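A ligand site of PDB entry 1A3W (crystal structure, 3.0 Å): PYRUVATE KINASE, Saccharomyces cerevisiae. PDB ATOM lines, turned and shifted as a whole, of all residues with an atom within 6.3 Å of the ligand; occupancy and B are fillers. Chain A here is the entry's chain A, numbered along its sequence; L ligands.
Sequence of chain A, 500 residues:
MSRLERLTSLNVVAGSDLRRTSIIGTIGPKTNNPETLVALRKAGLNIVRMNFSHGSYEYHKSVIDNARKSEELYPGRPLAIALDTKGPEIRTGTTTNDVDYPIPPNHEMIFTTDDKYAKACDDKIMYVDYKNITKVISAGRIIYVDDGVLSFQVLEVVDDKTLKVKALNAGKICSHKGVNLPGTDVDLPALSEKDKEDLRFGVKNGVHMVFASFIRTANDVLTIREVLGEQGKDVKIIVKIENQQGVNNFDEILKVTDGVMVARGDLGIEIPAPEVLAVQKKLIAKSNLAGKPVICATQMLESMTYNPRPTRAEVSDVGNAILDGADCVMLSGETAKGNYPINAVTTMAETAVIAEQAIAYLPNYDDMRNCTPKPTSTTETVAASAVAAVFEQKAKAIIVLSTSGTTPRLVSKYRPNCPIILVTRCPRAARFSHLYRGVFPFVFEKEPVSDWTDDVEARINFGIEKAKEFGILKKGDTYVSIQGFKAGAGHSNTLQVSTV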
ATOM      1  N   THR A 379     -18.495  -4.071 -12.225  1.00  0.00           N
ATOM      2  CA  THR A 379     -17.543  -2.989 -12.021  1.00  0.00           C
ATOM      3  C   THR A 379     -18.176  -1.617 -12.261  1.00  0.00           C
ATOM      4  O   THR A 379     -17.774  -0.624 -11.660  1.00  0.00           O
ATOM      5  CB  THR A 379     -16.274  -3.188 -12.909  1.00  0.00           C
ATOM      6  OG1 THR A 379     -15.656  -1.922 -13.163  1.00  0.00           O
ATOM      7  CG2 THR A 379     -16.627  -3.845 -14.225  1.00  0.00           C
ATOM      8  N   VAL A 400      -8.973   4.582  -6.220  1.00  0.00           N
ATOM      9  CA  VAL A 400      -9.270   3.385  -6.993  1.00  0.00           C
ATOM     10  C   VAL A 400      -8.022   2.850  -7.681  1.00  0.00           C
ATOM     11  O   VAL A 400      -7.390   3.546  -8.473  1.00  0.00           O
ATOM     12  CB  VAL A 400     -10.347   3.666  -8.069  1.00  0.00           C
ATOM     13  CG1 VAL A 400     -10.114   5.031  -8.694  1.00  0.00           C
ATOM     14  CG2 VAL A 400     -10.297   2.596  -9.154  1.00  0.00           C
ATOM     15  N   LEU A 401      -7.678   1.610  -7.364  1.00  0.00           N
ATOM     16  CA  LEU A 401      -6.527   0.989  -7.988  1.00  0.00           C
ATOM     17  C   LEU A 401      -7.025   0.104  -9.125  1.00  0.00           C
ATOM     18  O   LEU A 401      -8.054  -0.554  -9.011  1.00  0.00           O
ATOM     19  CB  LEU A 401      -5.752   0.140  -6.969  1.00  0.00           C
ATOM     20  CG  LEU A 401      -6.467  -0.413  -5.726  1.00  0.00           C
ATOM     21  CD1 LEU A 401      -6.493  -1.932  -5.787  1.00  0.00           C
ATOM     22  CD2 LEU A 401      -5.749   0.047  -4.468  1.00  0.00           C
ATOM     23  N   SER A 402      -6.293   0.113 -10.227  1.00  0.00           N
ATOM     24  CA  SER A 402      -6.657  -0.697 -11.379  1.00  0.00           C
ATOM     25  C   SER A 402      -5.447  -0.856 -12.278  1.00  0.00           C
ATOM     26  O   SER A 402      -4.519  -0.052 -12.215  1.00  0.00           O
ATOM     27  CB  SER A 402      -7.790  -0.039 -12.142  1.00  0.00           C
ATOM     28  OG  SER A 402      -7.483   0.051 -13.524  1.00  0.00           O
ATOM     29  N   THR A 403      -5.449  -1.897 -13.097  1.00  0.00           N
ATOM     30  CA  THR A 403      -4.326  -2.165 -13.990  1.00  0.00           C
ATOM     31  C   THR A 403      -4.668  -2.036 -15.472  1.00  0.00           C
ATOM     32  O   THR A 403      -3.770  -1.937 -16.314  1.00  0.00           O
ATOM     33  CB  THR A 403      -3.751  -3.576 -13.736  1.00  0.00           C
ATOM     34  OG1 THR A 403      -4.219  -4.477 -14.742  1.00  0.00           O
ATOM     35  CG2 THR A 403      -4.170  -4.089 -12.360  1.00  0.00           C
ATOM     36  N   SER A 404      -5.955  -2.051 -15.792  1.00  0.00           N
ATOM     37  CA  SER A 404      -6.408  -1.939 -17.183  1.00  0.00           C
ATOM     38  C   SER A 404      -7.055  -0.583 -17.448  1.00  0.00           C
ATOM     39  O   SER A 404      -7.415  -0.271 -18.587  1.00  0.00           O
ATOM     40  CB  SER A 404      -7.405  -3.053 -17.487  1.00  0.00           C
ATOM     41  OG  SER A 404      -8.548  -2.552 -18.148  1.00  0.00           O
ATOM     42  N   GLY A 405      -7.186   0.215 -16.394  1.00  0.00           N
ATOM     43  CA  GLY A 405      -7.786   1.524 -16.535  1.00  0.00           C
ATOM     44  C   GLY A 405      -9.295   1.468 -16.524  1.00  0.00           C
ATOM     45  O   GLY A 405      -9.961   2.472 -16.256  1.00  0.00           O
ATOM     46  N   THR A 406      -9.848   0.296 -16.805  1.00  0.00           N
ATOM     47  CA  THR A 406     -11.289   0.089 -16.846  1.00  0.00           C
ATOM     48  C   THR A 406     -12.044   0.727 -15.685  1.00  0.00           C
ATOM     49  O   THR A 406     -12.828   1.660 -15.887  1.00  0.00           O
ATOM     50  CB  THR A 406     -11.637  -1.411 -16.850  1.00  0.00           C
ATOM     51  OG1 THR A 406     -11.199  -2.003 -18.070  1.00  0.00           O
ATOM     52  CG2 THR A 406     -13.130  -1.607 -16.703  1.00  0.00           C
ATOM     53  N   THR A 407     -11.807   0.239 -14.479  1.00  0.00           N
ATOM     54  CA  THR A 407     -12.482   0.754 -13.294  1.00  0.00           C
ATOM     55  C   THR A 407     -12.464   2.284 -13.175  1.00  0.00           C
ATOM     56  O   THR A 407     -13.513   2.928 -13.133  1.00  0.00           O
ATOM     57  CB  THR A 407     -11.893   0.153 -11.991  1.00  0.00           C
ATOM     58  OG1 THR A 407     -12.184  -1.247 -11.936  1.00  0.00           O
ATOM     59  CG2 THR A 407     -12.487   0.839 -10.780  1.00  0.00           C
ATOM     60  N   PRO A 408     -11.259   2.887 -13.146  1.00  0.00           N
ATOM     61  CA  PRO A 408     -11.205   4.344 -13.026  1.00  0.00           C
ATOM     62  C   PRO A 408     -12.001   5.029 -14.139  1.00  0.00           C
ATOM     63  O   PRO A 408     -12.414   6.179 -14.012  1.00  0.00           O
ATOM     64  CB  PRO A 408      -9.712   4.666 -13.101  1.00  0.00           C
ATOM     65  CG  PRO A 408      -9.095   3.453 -13.716  1.00  0.00           C
ATOM     66  CD  PRO A 408      -9.919   2.298 -13.255  1.00  0.00           C
ATOM     67  N   ARG A 425       0.272  -0.009 -10.870  1.00  0.00           N
ATOM     68  CA  ARG A 425       1.617  -0.521 -11.049  1.00  0.00           C
ATOM     69  C   ARG A 425       2.000  -0.256 -12.494  1.00  0.00           C
ATOM     70  O   ARG A 425       3.108   0.179 -12.790  1.00  0.00           O
ATOM     71  CB  ARG A 425       1.662  -2.022 -10.769  1.00  0.00           C
ATOM     72  CG  ARG A 425       1.171  -2.432  -9.390  1.00  0.00           C
ATOM     73  CD  ARG A 425       2.076  -3.500  -8.763  1.00  0.00           C
ATOM     74  NE  ARG A 425       2.588  -3.079  -7.461  1.00  0.00           N
ATOM     75  CZ  ARG A 425       2.179  -3.588  -6.301  1.00  0.00           C
ATOM     76  NH1 ARG A 425       1.251  -4.538  -6.290  1.00  0.00           N
ATOM     77  NH2 ARG A 425       2.685  -3.146  -5.161  1.00  0.00           N
ATOM     78  N   TRP A 452      -3.008 -10.340  -1.550  1.00  0.00           N
ATOM     79  CA  TRP A 452      -3.892  -9.525  -2.380  1.00  0.00           C
ATOM     80  C   TRP A 452      -4.854  -8.859  -1.400  1.00  0.00           C
ATOM     81  O   TRP A 452      -5.922  -8.378  -1.787  1.00  0.00           O
ATOM     82  CB  TRP A 452      -4.684 -10.429  -3.334  1.00  0.00           C
ATOM     83  CG  TRP A 452      -5.320  -9.741  -4.519  1.00  0.00           C
ATOM     84  CD1 TRP A 452      -5.151  -8.441  -4.903  1.00  0.00           C
ATOM     85  CD2 TRP A 452      -6.185 -10.333  -5.495  1.00  0.00           C
ATOM     86  NE1 TRP A 452      -5.851  -8.191  -6.049  1.00  0.00           N
ATOM     87  CE2 TRP A 452      -6.501  -9.332  -6.444  1.00  0.00           C
ATOM     88  CE3 TRP A 452      -6.738 -11.618  -5.671  1.00  0.00           C
ATOM     89  CZ2 TRP A 452      -7.338  -9.568  -7.549  1.00  0.00           C
ATOM     90  CZ3 TRP A 452      -7.570 -11.846  -6.772  1.00  0.00           C
ATOM     91  CH2 TRP A 452      -7.855 -10.827  -7.695  1.00  0.00           C
ATOM     92  N   ASP A 455      -1.424  -6.050   0.183  1.00  0.00           N
ATOM     93  CA  ASP A 455      -0.832  -5.290  -0.901  1.00  0.00           C
ATOM     94  C   ASP A 455      -1.783  -4.181  -1.354  1.00  0.00           C
ATOM     95  O   ASP A 455      -1.443  -3.000  -1.325  1.00  0.00           O
ATOM     96  CB  ASP A 455      -0.521  -6.202  -2.069  1.00  0.00           C
ATOM     97  CG  ASP A 455       0.181  -5.492  -3.194  1.00  0.00           C
ATOM     98  OD1 ASP A 455       1.183  -4.799  -2.923  1.00  0.00           O
ATOM     99  OD2 ASP A 455      -0.276  -5.621  -4.343  1.00  0.00           O
ATOM    100  N   VAL A 456      -2.982  -4.579  -1.765  1.00  0.00           N
ATOM    101  CA  VAL A 456      -3.993  -3.625  -2.227  1.00  0.00           C
ATOM    102  C   VAL A 456      -4.166  -2.553  -1.180  1.00  0.00           C
ATOM    103  O   VAL A 456      -4.351  -1.378  -1.493  1.00  0.00           O
ATOM    104  CB  VAL A 456      -5.361  -4.313  -2.462  1.00  0.00           C
ATOM    105  CG1 VAL A 456      -5.154  -5.646  -3.157  1.00  0.00           C
ATOM    106  CG2 VAL A 456      -6.082  -4.510  -1.136  1.00  0.00           C
ATOM    107  N   ARG A 459      -1.449  -0.275  -1.026  1.00  0.00           N
ATOM    108  CA  ARG A 459      -1.627   0.476  -2.255  1.00  0.00           C
ATOM    109  C   ARG A 459      -2.662   1.573  -1.986  1.00  0.00           C
ATOM    110  O   ARG A 459      -2.449   2.727  -2.341  1.00  0.00           O
ATOM    111  CB  ARG A 459      -2.136  -0.449  -3.357  1.00  0.00           C
ATOM    112  CG  ARG A 459      -1.343  -0.399  -4.632  1.00  0.00           C
ATOM    113  CD  ARG A 459      -1.034  -1.800  -5.178  1.00  0.00           C
ATOM    114  NE  ARG A 459      -2.062  -2.784  -4.834  1.00  0.00           N
ATOM    115  CZ  ARG A 459      -2.561  -3.661  -5.697  1.00  0.00           C
ATOM    116  NH1 ARG A 459      -2.138  -3.678  -6.963  1.00  0.00           N
ATOM    117  NH2 ARG A 459      -3.490  -4.522  -5.309  1.00  0.00           N
ATOM    118  N   ILE A 482     -12.090   1.792  -4.001  1.00  0.00           N
ATOM    119  CA  ILE A 482     -12.672   0.831  -4.925  1.00  0.00           C
ATOM    120  C   ILE A 482     -11.680  -0.286  -5.228  1.00  0.00           C
ATOM    121  O   ILE A 482     -10.595  -0.024  -5.757  1.00  0.00           O
ATOM    122  CB  ILE A 482     -13.087   1.507  -6.239  1.00  0.00           C
ATOM    123  CG1 ILE A 482     -13.900   2.772  -5.943  1.00  0.00           C
ATOM    124  CG2 ILE A 482     -13.914   0.556  -7.076  1.00  0.00           C
ATOM    125  CD1 ILE A 482     -14.404   3.479  -7.179  1.00  0.00           C
ATOM    126  N   GLN A 483     -12.061  -1.513  -4.896  1.00  0.00           N
ATOM    127  CA  GLN A 483     -11.231  -2.684  -5.126  1.00  0.00           C
ATOM    128  C   GLN A 483     -12.105  -3.900  -5.396  1.00  0.00           C
ATOM    129  O   GLN A 483     -13.292  -3.889  -5.105  1.00  0.00           O
ATOM    130  CB  GLN A 483     -10.351  -2.963  -3.905  1.00  0.00           C
ATOM    131  CG  GLN A 483     -11.119  -3.089  -2.613  1.00  0.00           C
ATOM    132  CD  GLN A 483     -10.259  -3.548  -1.463  1.00  0.00           C
ATOM    133  OE1 GLN A 483     -10.555  -4.531  -0.791  1.00  0.00           O
ATOM    134  NE2 GLN A 483      -9.172  -2.832  -1.226  1.00  0.00           N
ATOM    135  N   GLY A 484     -11.496  -4.945  -5.937  1.00  0.00           N
ATOM    136  CA  GLY A 484     -12.259  -6.154  -6.239  1.00  0.00           C
ATOM    137  C   GLY A 484     -11.944  -7.332  -5.360  1.00  0.00           C
ATOM    138  O   GLY A 484     -11.137  -7.237  -4.425  1.00  0.00           O
ATOM    139  N   PHE A 485     -12.588  -8.455  -5.660  1.00  0.00           N
ATOM    140  CA  PHE A 485     -12.397  -9.685  -4.903  1.00  0.00           C
ATOM    141  C   PHE A 485     -13.448 -10.749  -5.263  1.00  0.00           C
ATOM    142  O   PHE A 485     -14.024 -11.375  -4.381  1.00  0.00           O
ATOM    143  CB  PHE A 485     -12.462  -9.406  -3.395  1.00  0.00           C
ATOM    144  CG  PHE A 485     -11.736 -10.415  -2.563  1.00  0.00           C
ATOM    145  CD1 PHE A 485     -10.361 -10.606  -2.726  1.00  0.00           C
ATOM    146  CD2 PHE A 485     -12.412 -11.183  -1.628  1.00  0.00           C
ATOM    147  CE1 PHE A 485      -9.684 -11.569  -1.971  1.00  0.00           C
ATOM    148  CE2 PHE A 485     -11.740 -12.148  -0.865  1.00  0.00           C
ATOM    149  CZ  PHE A 485     -10.370 -12.339  -1.044  1.00  0.00           C
ATOM    150  N   ALA A 489     -11.801 -14.792 -10.837  1.00  0.00           N
ATOM    151  CA  ALA A 489     -11.741 -13.667 -11.767  1.00  0.00           C
ATOM    152  C   ALA A 489     -12.091 -12.313 -11.146  1.00  0.00           C
ATOM    153  O   ALA A 489     -12.776 -11.487 -11.769  1.00  0.00           O
ATOM    154  CB  ALA A 489     -12.673 -13.952 -12.962  1.00  0.00           C
ATOM    155  N   GLY A 490     -11.597 -12.071  -9.938  1.00  0.00           N
ATOM    156  CA  GLY A 490     -11.878 -10.807  -9.271  1.00  0.00           C
ATOM    157  C   GLY A 490     -11.668  -9.634 -10.209  1.00  0.00           C
ATOM    158  O   GLY A 490     -10.709  -9.620 -10.985  1.00  0.00           O
ATOM    159  N   HIS A 491     -12.588  -8.665 -10.142  1.00  0.00           N
ATOM    160  CA  HIS A 491     -12.523  -7.479 -10.983  1.00  0.00           C
ATOM    161  C   HIS A 491     -13.426  -6.362 -10.479  1.00  0.00           C
ATOM    162  O   HIS A 491     -14.419  -6.008 -11.120  1.00  0.00           O
ATOM    163  CB  HIS A 491     -12.894  -7.824 -12.419  1.00  0.00           C
ATOM    164  CG  HIS A 491     -11.726  -7.809 -13.355  1.00  0.00           C
ATOM    165  ND1 HIS A 491     -11.322  -8.935 -14.046  1.00  0.00           N
ATOM    166  CD2 HIS A 491     -10.873  -6.827 -13.701  1.00  0.00           C
ATOM    167  CE1 HIS A 491     -10.264  -8.632 -14.774  1.00  0.00           C
ATOM    168  NE2 HIS A 491      -9.969  -7.351 -14.585  1.00  0.00           N
ATOM    169  N   SER A 492     -13.065  -5.797  -9.323  1.00  0.00           N
ATOM    170  CA  SER A 492     -13.818  -4.709  -8.716  1.00  0.00           C
ATOM    171  C   SER A 492     -15.272  -5.077  -8.421  1.00  0.00           C
ATOM    172  O   SER A 492     -16.029  -5.495  -9.314  1.00  0.00           O
ATOM    173  CB  SER A 492     -13.775  -3.460  -9.599  1.00  0.00           C
ATOM    174  OG  SER A 492     -12.858  -3.605 -10.681  1.00  0.00           O
HETATM  175  P1  LIG L   1      -4.162  -6.402  -8.327  1.00  0.00           P
HETATM  176  O1  LIG L   1      -3.872  -7.591  -9.174  1.00  0.00           O
HETATM  177  O2  LIG L   1      -3.410  -5.229  -8.837  1.00  0.00           O
HETATM  178  O3  LIG L   1      -3.832  -6.681  -6.906  1.00  0.00           O
HETATM  179  O4  LIG L   1      -5.719  -6.109  -8.428  1.00  0.00           O
HETATM  180  C1  LIG L   1      -6.344  -5.070  -7.662  1.00  0.00           C
HETATM  181  C2  LIG L   1      -7.628  -4.655  -8.391  1.00  0.00           C
HETATM  182  O5  LIG L   1      -8.288  -3.613  -7.662  1.00  0.00           O
HETATM  183  C3  LIG L   1      -8.571  -5.859  -8.572  1.00  0.00           C
HETATM  184  O6  LIG L   1      -9.385  -6.135  -7.463  1.00  0.00           O
HETATM  185  C4  LIG L   1      -9.381  -5.509  -9.804  1.00  0.00           C
HETATM  186  O7  LIG L   1      -9.716  -6.693 -10.540  1.00  0.00           O
HETATM  187  C5  LIG L   1      -8.348  -4.689 -10.621  1.00  0.00           C
HETATM  188  O8  LIG L   1      -7.318  -4.193  -9.729  1.00  0.00           O
HETATM  189  C6  LIG L   1      -8.979  -3.497 -11.328  1.00  0.00           C
HETATM  190  O9  LIG L   1      -9.360  -3.900 -12.656  1.00  0.00           O
HETATM  191  P2  LIG L   1      -9.216  -2.848 -13.850  1.00  0.00           P
HETATM  192  O10 LIG L   1     -10.034  -1.658 -13.534  1.00  0.00           O
HETATM  193  O11 LIG L   1      -7.789  -2.478 -13.989  1.00  0.00           O
HETATM  194  O12 LIG L   1      -9.675  -3.476 -15.113  1.00  0.00           O
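An oxygen (O10) of the ligand sits at hydrogen-bond distance from the side-chain hydroxyl (OG1) of Thr 407.
The backbone NH of Thr 403 sits at hydrogen-bond distance from an oxygen (O11) of the ligand, 2.6 Å away.
The backbone NH (N) of Thr 407 sits at hydrogen-bond distance from an oxygen (O10) of the ligand (2.8 Å).
An oxygen (O11) of the ligand sits at hydrogen-bond distance from the backbone NH (N) of Ser 404 (2.6 Å).
The backbone NH (N) of Gly 484 is in hydrogen-bond range of an oxygen (O6) of the ligand (2.9 Å).
The backbone carbonyl oxygen (O) of Leu 401 sits close to an oxygen (O5) of the ligand (3.4 Å).
The side-chain hydroxyl of Ser 402 lies within hydrogen-bond range of an oxygen (O11) of the ligand (2.6 Å).
O7 of the ligand lies within hydrogen-bond range of O of Gly 490 (3.1 Å).
The side-chain hydroxyl (OG) of Ser 404 sits close to an oxygen (O12) of the ligand (3.4 Å).
An oxygen (O3) of the ligand lies within salt-bridge range of the guanidinium group (NH2) of Arg 459, 2.7 Å away.
An oxygen (O3) of the ligand is in hydrogen-bond range of the indole nitrogen (NE1) of Trp 452, 2.7 Å away.
The guanidinium group of Arg 459 is in salt-bridge range of the side-chain carboxylate of Asp 455 (3.4 Å).
The side-chain hydroxyl (OG) of Ser 402 sits at hydrogen-bond distance from the backbone NH (N) of Gly 405 (2.9 Å).
The side-chain hydroxyl of Ser 402 is in hydrogen-bond range of the backbone NH of Ser 404, at 3.4 Å.
OG of Ser 492 lies within hydrogen-bond range of OG1 of Thr 407 (2.8 Å).
OG1 of Thr 406 is in hydrogen-bond range of OG of Ser 404 (2.7 Å).
Gly 405 touches the ligand (N to O11, 3.7 Å).
CB of Thr 406 touches O12 of the ligand, at 3.3 Å.
Pro 408 touches the ligand (CD to O10, 3.97 Å).
Gln 483 touches the ligand (CA to O5, 3.99 Å).
His 491 touches the ligand (CA to O7, 2.9 Å).
N of Ser 492 touches O7 of the ligand (3.7 Å).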
